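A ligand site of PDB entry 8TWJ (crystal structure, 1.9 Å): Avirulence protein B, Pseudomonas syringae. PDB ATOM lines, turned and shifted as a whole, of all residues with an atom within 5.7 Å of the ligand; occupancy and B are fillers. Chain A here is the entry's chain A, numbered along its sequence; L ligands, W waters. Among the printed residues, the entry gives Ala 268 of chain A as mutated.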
ATOM      1  N   GLY A  48     -25.178 -26.778 -28.857  1.00  0.00           N
ATOM      2  CA  GLY A  48     -24.848 -26.067 -27.630  1.00  0.00           C
ATOM      3  C   GLY A  48     -24.034 -26.884 -26.631  1.00  0.00           C
ATOM      4  O   GLY A  48     -23.726 -26.378 -25.549  1.00  0.00           O
ATOM      5  N   ALA A  49     -23.655 -28.102 -26.965  1.00  0.00           N
ATOM      6  CA  ALA A  49     -22.845 -28.877 -26.036  1.00  0.00           C
ATOM      7  C   ALA A  49     -21.389 -28.402 -26.050  1.00  0.00           C
ATOM      8  O   ALA A  49     -20.901 -27.884 -27.049  1.00  0.00           O
ATOM      9  CB  ALA A  49     -22.855 -30.365 -26.382  1.00  0.00           C
ATOM     10  N   ALA A  50     -20.692 -28.606 -24.941  1.00  0.00           N
ATOM     11  CA  ALA A  50     -19.260 -28.293 -24.871  1.00  0.00           C
ATOM     12  C   ALA A  50     -18.538 -29.623 -24.936  1.00  0.00           C
ATOM     13  O   ALA A  50     -18.377 -30.295 -23.919  1.00  0.00           O
ATOM     14  CB  ALA A  50     -18.947 -27.523 -23.601  1.00  0.00           C
ATOM     15  N   LYS A  58     -20.002 -35.441 -20.375  1.00  0.00           N
ATOM     16  CA  LYS A  58     -21.150 -34.649 -19.928  1.00  0.00           C
ATOM     17  C   LYS A  58     -22.223 -34.582 -21.025  1.00  0.00           C
ATOM     18  O   LYS A  58     -23.421 -34.579 -20.721  1.00  0.00           O
ATOM     19  CB  LYS A  58     -20.708 -33.248 -19.497  1.00  0.00           C
ATOM     20  CG  LYS A  58     -21.872 -32.284 -19.255  1.00  0.00           C
ATOM     21  CD  LYS A  58     -21.480 -31.106 -18.349  1.00  0.00           C
ATOM     22  CE  LYS A  58     -22.588 -30.002 -18.281  1.00  0.00           C
ATOM     23  NZ  LYS A  58     -23.039 -29.714 -16.930  1.00  0.00           N
ATOM     24  N   GLU A  63     -29.650 -35.121 -18.989  1.00  0.00           N
ATOM     25  CA  GLU A  63     -29.843 -33.723 -18.634  1.00  0.00           C
ATOM     26  C   GLU A  63     -29.237 -32.819 -19.711  1.00  0.00           C
ATOM     27  O   GLU A  63     -29.849 -31.823 -20.142  1.00  0.00           O
ATOM     28  CB  GLU A  63     -29.203 -33.418 -17.291  1.00  0.00           C
ATOM     29  CG  GLU A  63     -29.847 -34.098 -16.075  1.00  0.00           C
ATOM     30  CD  GLU A  63     -29.797 -35.638 -16.103  1.00  0.00           C
ATOM     31  OE1 GLU A  63     -30.831 -36.276 -15.781  1.00  0.00           O
ATOM     32  OE2 GLU A  63     -28.727 -36.213 -16.471  1.00  0.00           O
ATOM     33  N   ASN A  64     -28.042 -33.175 -20.157  1.00  0.00           N
ATOM     34  CA  ASN A  64     -27.376 -32.381 -21.182  1.00  0.00           C
ATOM     35  C   ASN A  64     -28.101 -32.501 -22.508  1.00  0.00           C
ATOM     36  O   ASN A  64     -28.186 -31.531 -23.277  1.00  0.00           O
ATOM     37  CB  ASN A  64     -25.934 -32.817 -21.336  1.00  0.00           C
ATOM     38  CG  ASN A  64     -25.034 -31.643 -21.701  1.00  0.00           C
ATOM     39  OD1 ASN A  64     -24.796 -30.778 -20.874  1.00  0.00           O
ATOM     40  ND2 ASN A  64     -24.577 -31.574 -22.964  1.00  0.00           N
ATOM     41  N   TYR A  67     -31.006 -30.199 -22.354  1.00  0.00           N
ATOM     42  CA  TYR A  67     -30.527 -28.816 -22.486  1.00  0.00           C
ATOM     43  C   TYR A  67     -30.282 -28.476 -23.934  1.00  0.00           C
ATOM     44  O   TYR A  67     -30.739 -27.445 -24.437  1.00  0.00           O
ATOM     45  CB  TYR A  67     -29.251 -28.619 -21.658  1.00  0.00           C
ATOM     46  CG  TYR A  67     -28.463 -27.353 -21.861  1.00  0.00           C
ATOM     47  CD1 TYR A  67     -27.494 -27.263 -22.848  1.00  0.00           C
ATOM     48  CD2 TYR A  67     -28.629 -26.276 -21.017  1.00  0.00           C
ATOM     49  CE1 TYR A  67     -26.733 -26.107 -23.008  1.00  0.00           C
ATOM     50  CE2 TYR A  67     -27.873 -25.124 -21.165  1.00  0.00           C
ATOM     51  CZ  TYR A  67     -26.955 -25.041 -22.170  1.00  0.00           C
ATOM     52  OH  TYR A  67     -26.211 -23.896 -22.292  1.00  0.00           O
ATOM     53  N   CYS A  68     -29.586 -29.360 -24.643  1.00  0.00           N
ATOM     54  CA  CYS A  68     -29.219 -29.091 -26.024  1.00  0.00           C
ATOM     55  C   CYS A  68     -30.424 -29.059 -26.943  1.00  0.00           C
ATOM     56  O   CYS A  68     -30.489 -28.231 -27.852  1.00  0.00           O
ATOM     57  CB  CYS A  68     -28.240 -30.163 -26.498  1.00  0.00           C
ATOM     58  SG  CYS A  68     -26.561 -29.932 -25.781  1.00  0.00           S
ATOM     59  N   MET A  71     -32.166 -25.883 -26.542  1.00  0.00           N
ATOM     60  CA  MET A  71     -31.473 -24.822 -27.264  1.00  0.00           C
ATOM     61  C   MET A  71     -31.834 -24.850 -28.733  1.00  0.00           C
ATOM     62  O   MET A  71     -32.058 -23.810 -29.343  1.00  0.00           O
ATOM     63  CB  MET A  71     -29.944 -24.916 -27.135  1.00  0.00           C
ATOM     64  CG  MET A  71     -29.276 -23.557 -27.446  1.00  0.00           C
ATOM     65  SD  MET A  71     -27.505 -23.508 -27.841  1.00  0.00           S
ATOM     66  CE  MET A  71     -26.918 -23.176 -26.207  1.00  0.00           C
ATOM     67  N   ARG A 101     -31.241 -19.175 -21.605  1.00  0.00           N
ATOM     68  CA  ARG A 101     -30.229 -19.779 -20.747  1.00  0.00           C
ATOM     69  C   ARG A 101     -30.636 -19.725 -19.286  1.00  0.00           C
ATOM     70  O   ARG A 101     -30.439 -20.689 -18.544  1.00  0.00           O
ATOM     71  CB  ARG A 101     -28.877 -19.089 -20.938  1.00  0.00           C
ATOM     72  CG  ARG A 101     -27.757 -19.653 -20.100  1.00  0.00           C
ATOM     73  CD  ARG A 101     -27.441 -21.119 -20.540  1.00  0.00           C
ATOM     74  NE  ARG A 101     -26.440 -21.762 -19.700  1.00  0.00           N
ATOM     75  CZ  ARG A 101     -26.715 -22.440 -18.603  1.00  0.00           C
ATOM     76  NH1 ARG A 101     -27.949 -22.498 -18.124  1.00  0.00           N
ATOM     77  NH2 ARG A 101     -25.743 -23.095 -17.982  1.00  0.00           N
ATOM     78  N   PHE A 115     -25.430 -14.990 -14.768  1.00  0.00           N
ATOM     79  CA  PHE A 115     -26.008 -15.346 -16.050  1.00  0.00           C
ATOM     80  C   PHE A 115     -26.906 -14.244 -16.588  1.00  0.00           C
ATOM     81  O   PHE A 115     -27.124 -14.178 -17.809  1.00  0.00           O
ATOM     82  CB  PHE A 115     -26.780 -16.669 -15.922  1.00  0.00           C
ATOM     83  CG  PHE A 115     -25.895 -17.871 -15.977  1.00  0.00           C
ATOM     84  CD1 PHE A 115     -25.568 -18.463 -17.196  1.00  0.00           C
ATOM     85  CD2 PHE A 115     -25.406 -18.435 -14.808  1.00  0.00           C
ATOM     86  CE1 PHE A 115     -24.737 -19.560 -17.236  1.00  0.00           C
ATOM     87  CE2 PHE A 115     -24.586 -19.568 -14.856  1.00  0.00           C
ATOM     88  CZ  PHE A 115     -24.224 -20.092 -16.070  1.00  0.00           C
ATOM     89  N   TYR A 133     -11.050 -27.258 -18.584  1.00  0.00           N
ATOM     90  CA  TYR A 133     -10.366 -26.519 -19.642  1.00  0.00           C
ATOM     91  C   TYR A 133      -8.944 -26.991 -19.921  1.00  0.00           C
ATOM     92  O   TYR A 133      -8.197 -26.276 -20.586  1.00  0.00           O
ATOM     93  CB  TYR A 133     -10.272 -25.040 -19.252  1.00  0.00           C
ATOM     94  CG  TYR A 133     -11.594 -24.340 -19.074  1.00  0.00           C
ATOM     95  CD1 TYR A 133     -12.298 -23.887 -20.151  1.00  0.00           C
ATOM     96  CD2 TYR A 133     -12.117 -24.114 -17.816  1.00  0.00           C
ATOM     97  CE1 TYR A 133     -13.521 -23.252 -20.004  1.00  0.00           C
ATOM     98  CE2 TYR A 133     -13.323 -23.479 -17.638  1.00  0.00           C
ATOM     99  CZ  TYR A 133     -14.020 -23.043 -18.740  1.00  0.00           C
ATOM    100  OH  TYR A 133     -15.228 -22.396 -18.567  1.00  0.00           O
ATOM    101  N   GLN A 267     -21.338 -11.951 -17.283  1.00  0.00           N
ATOM    102  CA  GLN A 267     -20.552 -12.548 -16.196  1.00  0.00           C
ATOM    103  C   GLN A 267     -20.595 -14.061 -16.275  1.00  0.00           C
ATOM    104  O   GLN A 267     -19.634 -14.719 -15.878  1.00  0.00           O
ATOM    105  CB  GLN A 267     -21.095 -12.041 -14.853  1.00  0.00           C
ATOM    106  CG  GLN A 267     -20.987 -10.528 -14.680  1.00  0.00           C
ATOM    107  CD  GLN A 267     -21.705 -10.008 -13.454  1.00  0.00           C
ATOM    108  OE1 GLN A 267     -22.073 -10.769 -12.579  1.00  0.00           O
ATOM    109  NE2 GLN A 267     -21.970  -8.696 -13.417  1.00  0.00           N
ATOM    110  N   ALA A 268     -21.663 -14.629 -16.837  1.00  0.00           N
ATOM    111  CA  ALA A 268     -21.678 -16.071 -17.083  1.00  0.00           C
ATOM    112  C   ALA A 268     -22.553 -16.344 -18.291  1.00  0.00           C
ATOM    113  O   ALA A 268     -23.414 -15.545 -18.638  1.00  0.00           O
ATOM    114  CB  ALA A 268     -22.158 -16.848 -15.845  1.00  0.00           C
ATOM    115  N   GLY A 269     -22.294 -17.490 -18.950  1.00  0.00           N
ATOM    116  CA  GLY A 269     -23.166 -17.988 -20.007  1.00  0.00           C
ATOM    117  C   GLY A 269     -22.890 -17.445 -21.395  1.00  0.00           C
ATOM    118  O   GLY A 269     -23.670 -17.730 -22.311  1.00  0.00           O
ATOM    119  N   SER A 270     -21.830 -16.653 -21.584  1.00  0.00           N
ATOM    120  CA  SER A 270     -21.622 -16.008 -22.859  1.00  0.00           C
ATOM    121  C   SER A 270     -21.431 -17.008 -23.990  1.00  0.00           C
ATOM    122  O   SER A 270     -21.836 -16.751 -25.118  1.00  0.00           O
ATOM    123  CB  SER A 270     -20.399 -15.089 -22.780  1.00  0.00           C
ATOM    124  OG  SER A 270     -20.667 -13.958 -21.976  1.00  0.00           O
ATOM    125  N   ALA A 271     -20.735 -18.109 -23.747  1.00  0.00           N
ATOM    126  CA  ALA A 271     -20.502 -19.065 -24.821  1.00  0.00           C
ATOM    127  C   ALA A 271     -21.809 -19.642 -25.351  1.00  0.00           C
ATOM    128  O   ALA A 271     -22.013 -19.749 -26.569  1.00  0.00           O
ATOM    129  CB  ALA A 271     -19.591 -20.177 -24.311  1.00  0.00           C
ATOM    130  N   ALA A 272     -22.729 -19.954 -24.441  1.00  0.00           N
ATOM    131  CA  ALA A 272     -24.035 -20.474 -24.864  1.00  0.00           C
ATOM    132  C   ALA A 272     -24.829 -19.417 -25.603  1.00  0.00           C
ATOM    133  O   ALA A 272     -25.461 -19.690 -26.625  1.00  0.00           O
ATOM    134  CB  ALA A 272     -24.802 -20.958 -23.645  1.00  0.00           C
ATOM    135  N   LYS A 273     -24.790 -18.191 -25.113  1.00  0.00           N
ATOM    136  CA  LYS A 273     -25.549 -17.128 -25.769  1.00  0.00           C
ATOM    137  C   LYS A 273     -25.002 -16.816 -27.151  1.00  0.00           C
ATOM    138  O   LYS A 273     -25.765 -16.532 -28.064  1.00  0.00           O
ATOM    139  CB  LYS A 273     -25.515 -15.890 -24.865  1.00  0.00           C
ATOM    140  CG  LYS A 273     -26.201 -16.146 -23.522  1.00  0.00           C
ATOM    141  CD  LYS A 273     -25.713 -15.158 -22.493  1.00  0.00           C
ATOM    142  CE  LYS A 273     -26.325 -15.408 -21.122  1.00  0.00           C
ATOM    143  NZ  LYS A 273     -25.616 -14.569 -20.150  1.00  0.00           N
ATOM    144  N   GLU A 275     -23.340 -18.889 -29.232  1.00  0.00           N
ATOM    145  CA  GLU A 275     -23.729 -19.976 -30.140  1.00  0.00           C
ATOM    146  C   GLU A 275     -25.227 -19.906 -30.464  1.00  0.00           C
ATOM    147  O   GLU A 275     -25.640 -20.028 -31.638  1.00  0.00           O
ATOM    148  CB  GLU A 275     -23.368 -21.325 -29.554  1.00  0.00           C
ATOM    149  CG  GLU A 275     -23.879 -22.461 -30.461  1.00  0.00           C
ATOM    150  CD  GLU A 275     -23.372 -23.844 -30.059  1.00  0.00           C
ATOM    151  OE1 GLU A 275     -22.646 -23.982 -29.031  1.00  0.00           O
ATOM    152  OE2 GLU A 275     -23.697 -24.822 -30.808  1.00  0.00           O
ATOM    153  N   VAL A 297     -14.824 -26.897 -29.120  1.00  0.00           N
ATOM    154  CA  VAL A 297     -15.635 -26.103 -28.201  1.00  0.00           C
ATOM    155  C   VAL A 297     -15.586 -24.695 -28.758  1.00  0.00           C
ATOM    156  O   VAL A 297     -14.514 -24.087 -28.812  1.00  0.00           O
ATOM    157  CB  VAL A 297     -15.075 -26.216 -26.780  1.00  0.00           C
ATOM    158  CG1 VAL A 297     -15.898 -25.399 -25.794  1.00  0.00           C
ATOM    159  CG2 VAL A 297     -15.041 -27.694 -26.359  1.00  0.00           C
ATOM    160  N   SER A 298     -16.742 -24.197 -29.237  1.00  0.00           N
ATOM    161  CA  SER A 298     -16.735 -23.110 -30.194  1.00  0.00           C
ATOM    162  C   SER A 298     -16.202 -21.821 -29.594  1.00  0.00           C
ATOM    163  O   SER A 298     -15.449 -21.101 -30.271  1.00  0.00           O
ATOM    164  CB  SER A 298     -18.139 -22.896 -30.738  1.00  0.00           C
ATOM    165  OG  SER A 298     -18.997 -22.554 -29.664  1.00  0.00           O
ATOM    166  N   ASP A 299     -16.567 -21.485 -28.350  1.00  0.00           N
ATOM    167  CA  ASP A 299     -16.084 -20.226 -27.791  1.00  0.00           C
ATOM    168  C   ASP A 299     -14.587 -20.259 -27.610  1.00  0.00           C
ATOM    169  O   ASP A 299     -13.910 -19.241 -27.778  1.00  0.00           O
ATOM    170  CB  ASP A 299     -16.748 -19.908 -26.456  1.00  0.00           C
ATOM    171  CG  ASP A 299     -16.531 -20.989 -25.368  1.00  0.00           C
ATOM    172  OD1 ASP A 299     -16.933 -22.148 -25.561  1.00  0.00           O
ATOM    173  OD2 ASP A 299     -15.971 -20.677 -24.294  1.00  0.00           O
HETATM  174  N1  LIG L   1     -23.494 -26.152 -21.492  1.00  0.00           N
HETATM  175  C1  LIG L   1     -23.815 -27.482 -21.643  1.00  0.00           C
HETATM  176  N2  LIG L   1     -24.680 -27.988 -20.702  1.00  0.00           N
HETATM  177  C2  LIG L   1     -25.239 -27.300 -19.642  1.00  0.00           C
HETATM  178  C3  LIG L   1     -24.863 -25.931 -19.551  1.00  0.00           C
HETATM  179  C4  LIG L   1     -24.012 -25.400 -20.458  1.00  0.00           C
HETATM  180  O1  LIG L   1     -23.351 -28.178 -22.547  1.00  0.00           O
HETATM  181  O2  LIG L   1     -25.989 -27.906 -18.848  1.00  0.00           O
HETATM  182  C5  LIG L   1     -22.599 -25.571 -22.485  1.00  0.00           C
HETATM  183  C6  LIG L   1     -23.057 -24.187 -22.985  1.00  0.00           C
HETATM  184  O3  LIG L   1     -24.021 -24.216 -24.038  1.00  0.00           O
HETATM  185  C7  LIG L   1     -21.704 -23.589 -23.397  1.00  0.00           C
HETATM  186  C8  LIG L   1     -20.771 -24.097 -22.296  1.00  0.00           C
HETATM  187  O4  LIG L   1     -21.330 -25.390 -21.875  1.00  0.00           O
HETATM  188  O5  LIG L   1     -21.304 -24.027 -24.721  1.00  0.00           O
HETATM  189  C9  LIG L   1     -20.630 -23.228 -21.060  1.00  0.00           C
HETATM  190  O6  LIG L   1     -19.999 -21.960 -21.334  1.00  0.00           O
HETATM  191  P1  LIG L   1     -20.753 -20.602 -21.000  1.00  0.00           P
HETATM  192  O7  LIG L   1     -19.775 -19.494 -21.212  1.00  0.00           O
HETATM  193  O8  LIG L   1     -22.108 -20.557 -21.727  1.00  0.00           O
HETATM  194  O9  LIG L   1     -21.118 -20.729 -19.470  1.00  0.00           O
HETATM  195  P2  LIG L   1     -20.205 -20.390 -18.224  1.00  0.00           P
HETATM  196  O10 LIG L   1     -20.819 -21.257 -17.108  1.00  0.00           O
HETATM  197  O11 LIG L   1     -18.793 -20.880 -18.668  1.00  0.00           O
HETATM  198  O12 LIG L   1     -20.239 -18.952 -17.889  1.00  0.00           O
HETATM  199  O   HOH W   1     -22.401 -22.673 -26.584  1.00  0.00           O
HETATM  200  O   HOH W   2     -23.052 -22.870 -17.842  1.00  0.00           O
HETATM  201  O   HOH W   3     -23.708 -21.841 -20.150  1.00  0.00           O
HETATM  202  O   HOH W   4     -20.575 -27.274 -19.904  1.00  0.00           O
HETATM  203  O   HOH W   5     -20.070 -23.413 -16.007  1.00  0.00           O
HETATM  204  O   HOH W   6     -21.706 -30.456 -22.799  1.00  0.00           O
HETATM  205  O   HOH W   7     -18.585 -17.974 -16.130  1.00  0.00           O
HETATM  206  O   HOH W   8     -19.303 -24.809 -26.121  1.00  0.00           O
HETATM  207  O   HOH W   9     -19.945 -19.370 -14.583  1.00  0.00           O
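CA of Ala 49 touches O1 of the ligand, at 3.6 Å.
Ala 50 touches the ligand (N to O1, 3.6 Å).
Lys 58 touches the ligand (CE to N2, 3.8 Å).
CE of Met 71 touches O3 of the ligand, 3.8 Å away.
Arg 101 touches the ligand.
Phe 115 touches the ligand.
Tyr 133 touches the ligand (OH to O11, 3.9 Å).
Ala 268 touches the ligand.
Ser 270 touches the ligand.
Hydrophobic or aromatic side chains that line the ligand: Ala 50, Tyr 67, Met 71, Phe 115, Ala 268, Ala 271 and Ala 272.
Within 4 Å of the ligand: Gly 48, Ala 49, Ala 50, Lys 58, Asn 64, Tyr 67, Met 71, Arg 101, Phe 115, Tyr 133, Ala 268, Gly 269, Ser 270, Ala 271 and Ala 272.
Water W1 lies within hydrogen-bond range of O5 of the ligand, OE1 of Glu 275, O of Ala 271 and N of Ala 272.
Water W3 bridges O8 of the ligand (2.6 Å) and NE of Arg 101 (2.8 Å).
Water W7 lies within hydrogen-bond range of an oxygen (O12) of the ligand (2.6 Å) and the backbone carbonyl oxygen of Gln 267 (3.4 Å).
Water W6 lies within hydrogen-bond range of O1 of the ligand, N of Ala 50 and ND2 of Asn 64.
Water W2 lies within hydrogen-bond range of NH2 of Arg 101 (2.7 Å) and O10 of the ligand (2.9 Å).
The side-chain carboxylate of Glu 275 sits at hydrogen-bond distance from the backbone NH of Gly 48, 3.1 Å away.
O of Asn 64 lies within hydrogen-bond range of SG of Cys 68 (3.4 Å).
OH of Tyr 67 lies within hydrogen-bond range of NE of Arg 101, 3.4 Å away.
The side-chain amino group of Lys 273 sits at hydrogen-bond distance from the backbone carbonyl oxygen of Ala 268.
The side-chain sulfur of Cys 68 is in hydrogen-bond range of the backbone NH of Ala 49, 3.6 Å away.
The backbone carbonyl oxygen (O) of Phe 115 lies within hydrogen-bond range of the side-chain amino group (NZ) of Lys 273, at 2.8 Å.
An oxygen (O3) of the ligand lies within hydrogen-bond range of the backbone carbonyl oxygen of Gly 48.
The backbone NH (N) of Gly 269 lies within hydrogen-bond range of an oxygen (O12) of the ligand (2.7 Å).
The side-chain amide oxygen (OD1) of Asn 64 is in hydrogen-bond range of a nitrogen (N2) of the ligand (2.8 Å).
OH of Tyr 67 sits at hydrogen-bond distance from O3 of the ligand (2.8 Å).
An oxygen (O8) of the ligand lies within hydrogen-bond range of the backbone NH (N) of Ala 272.
O7 of the ligand is in hydrogen-bond range of N of Ala 271 (3.0 Å).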
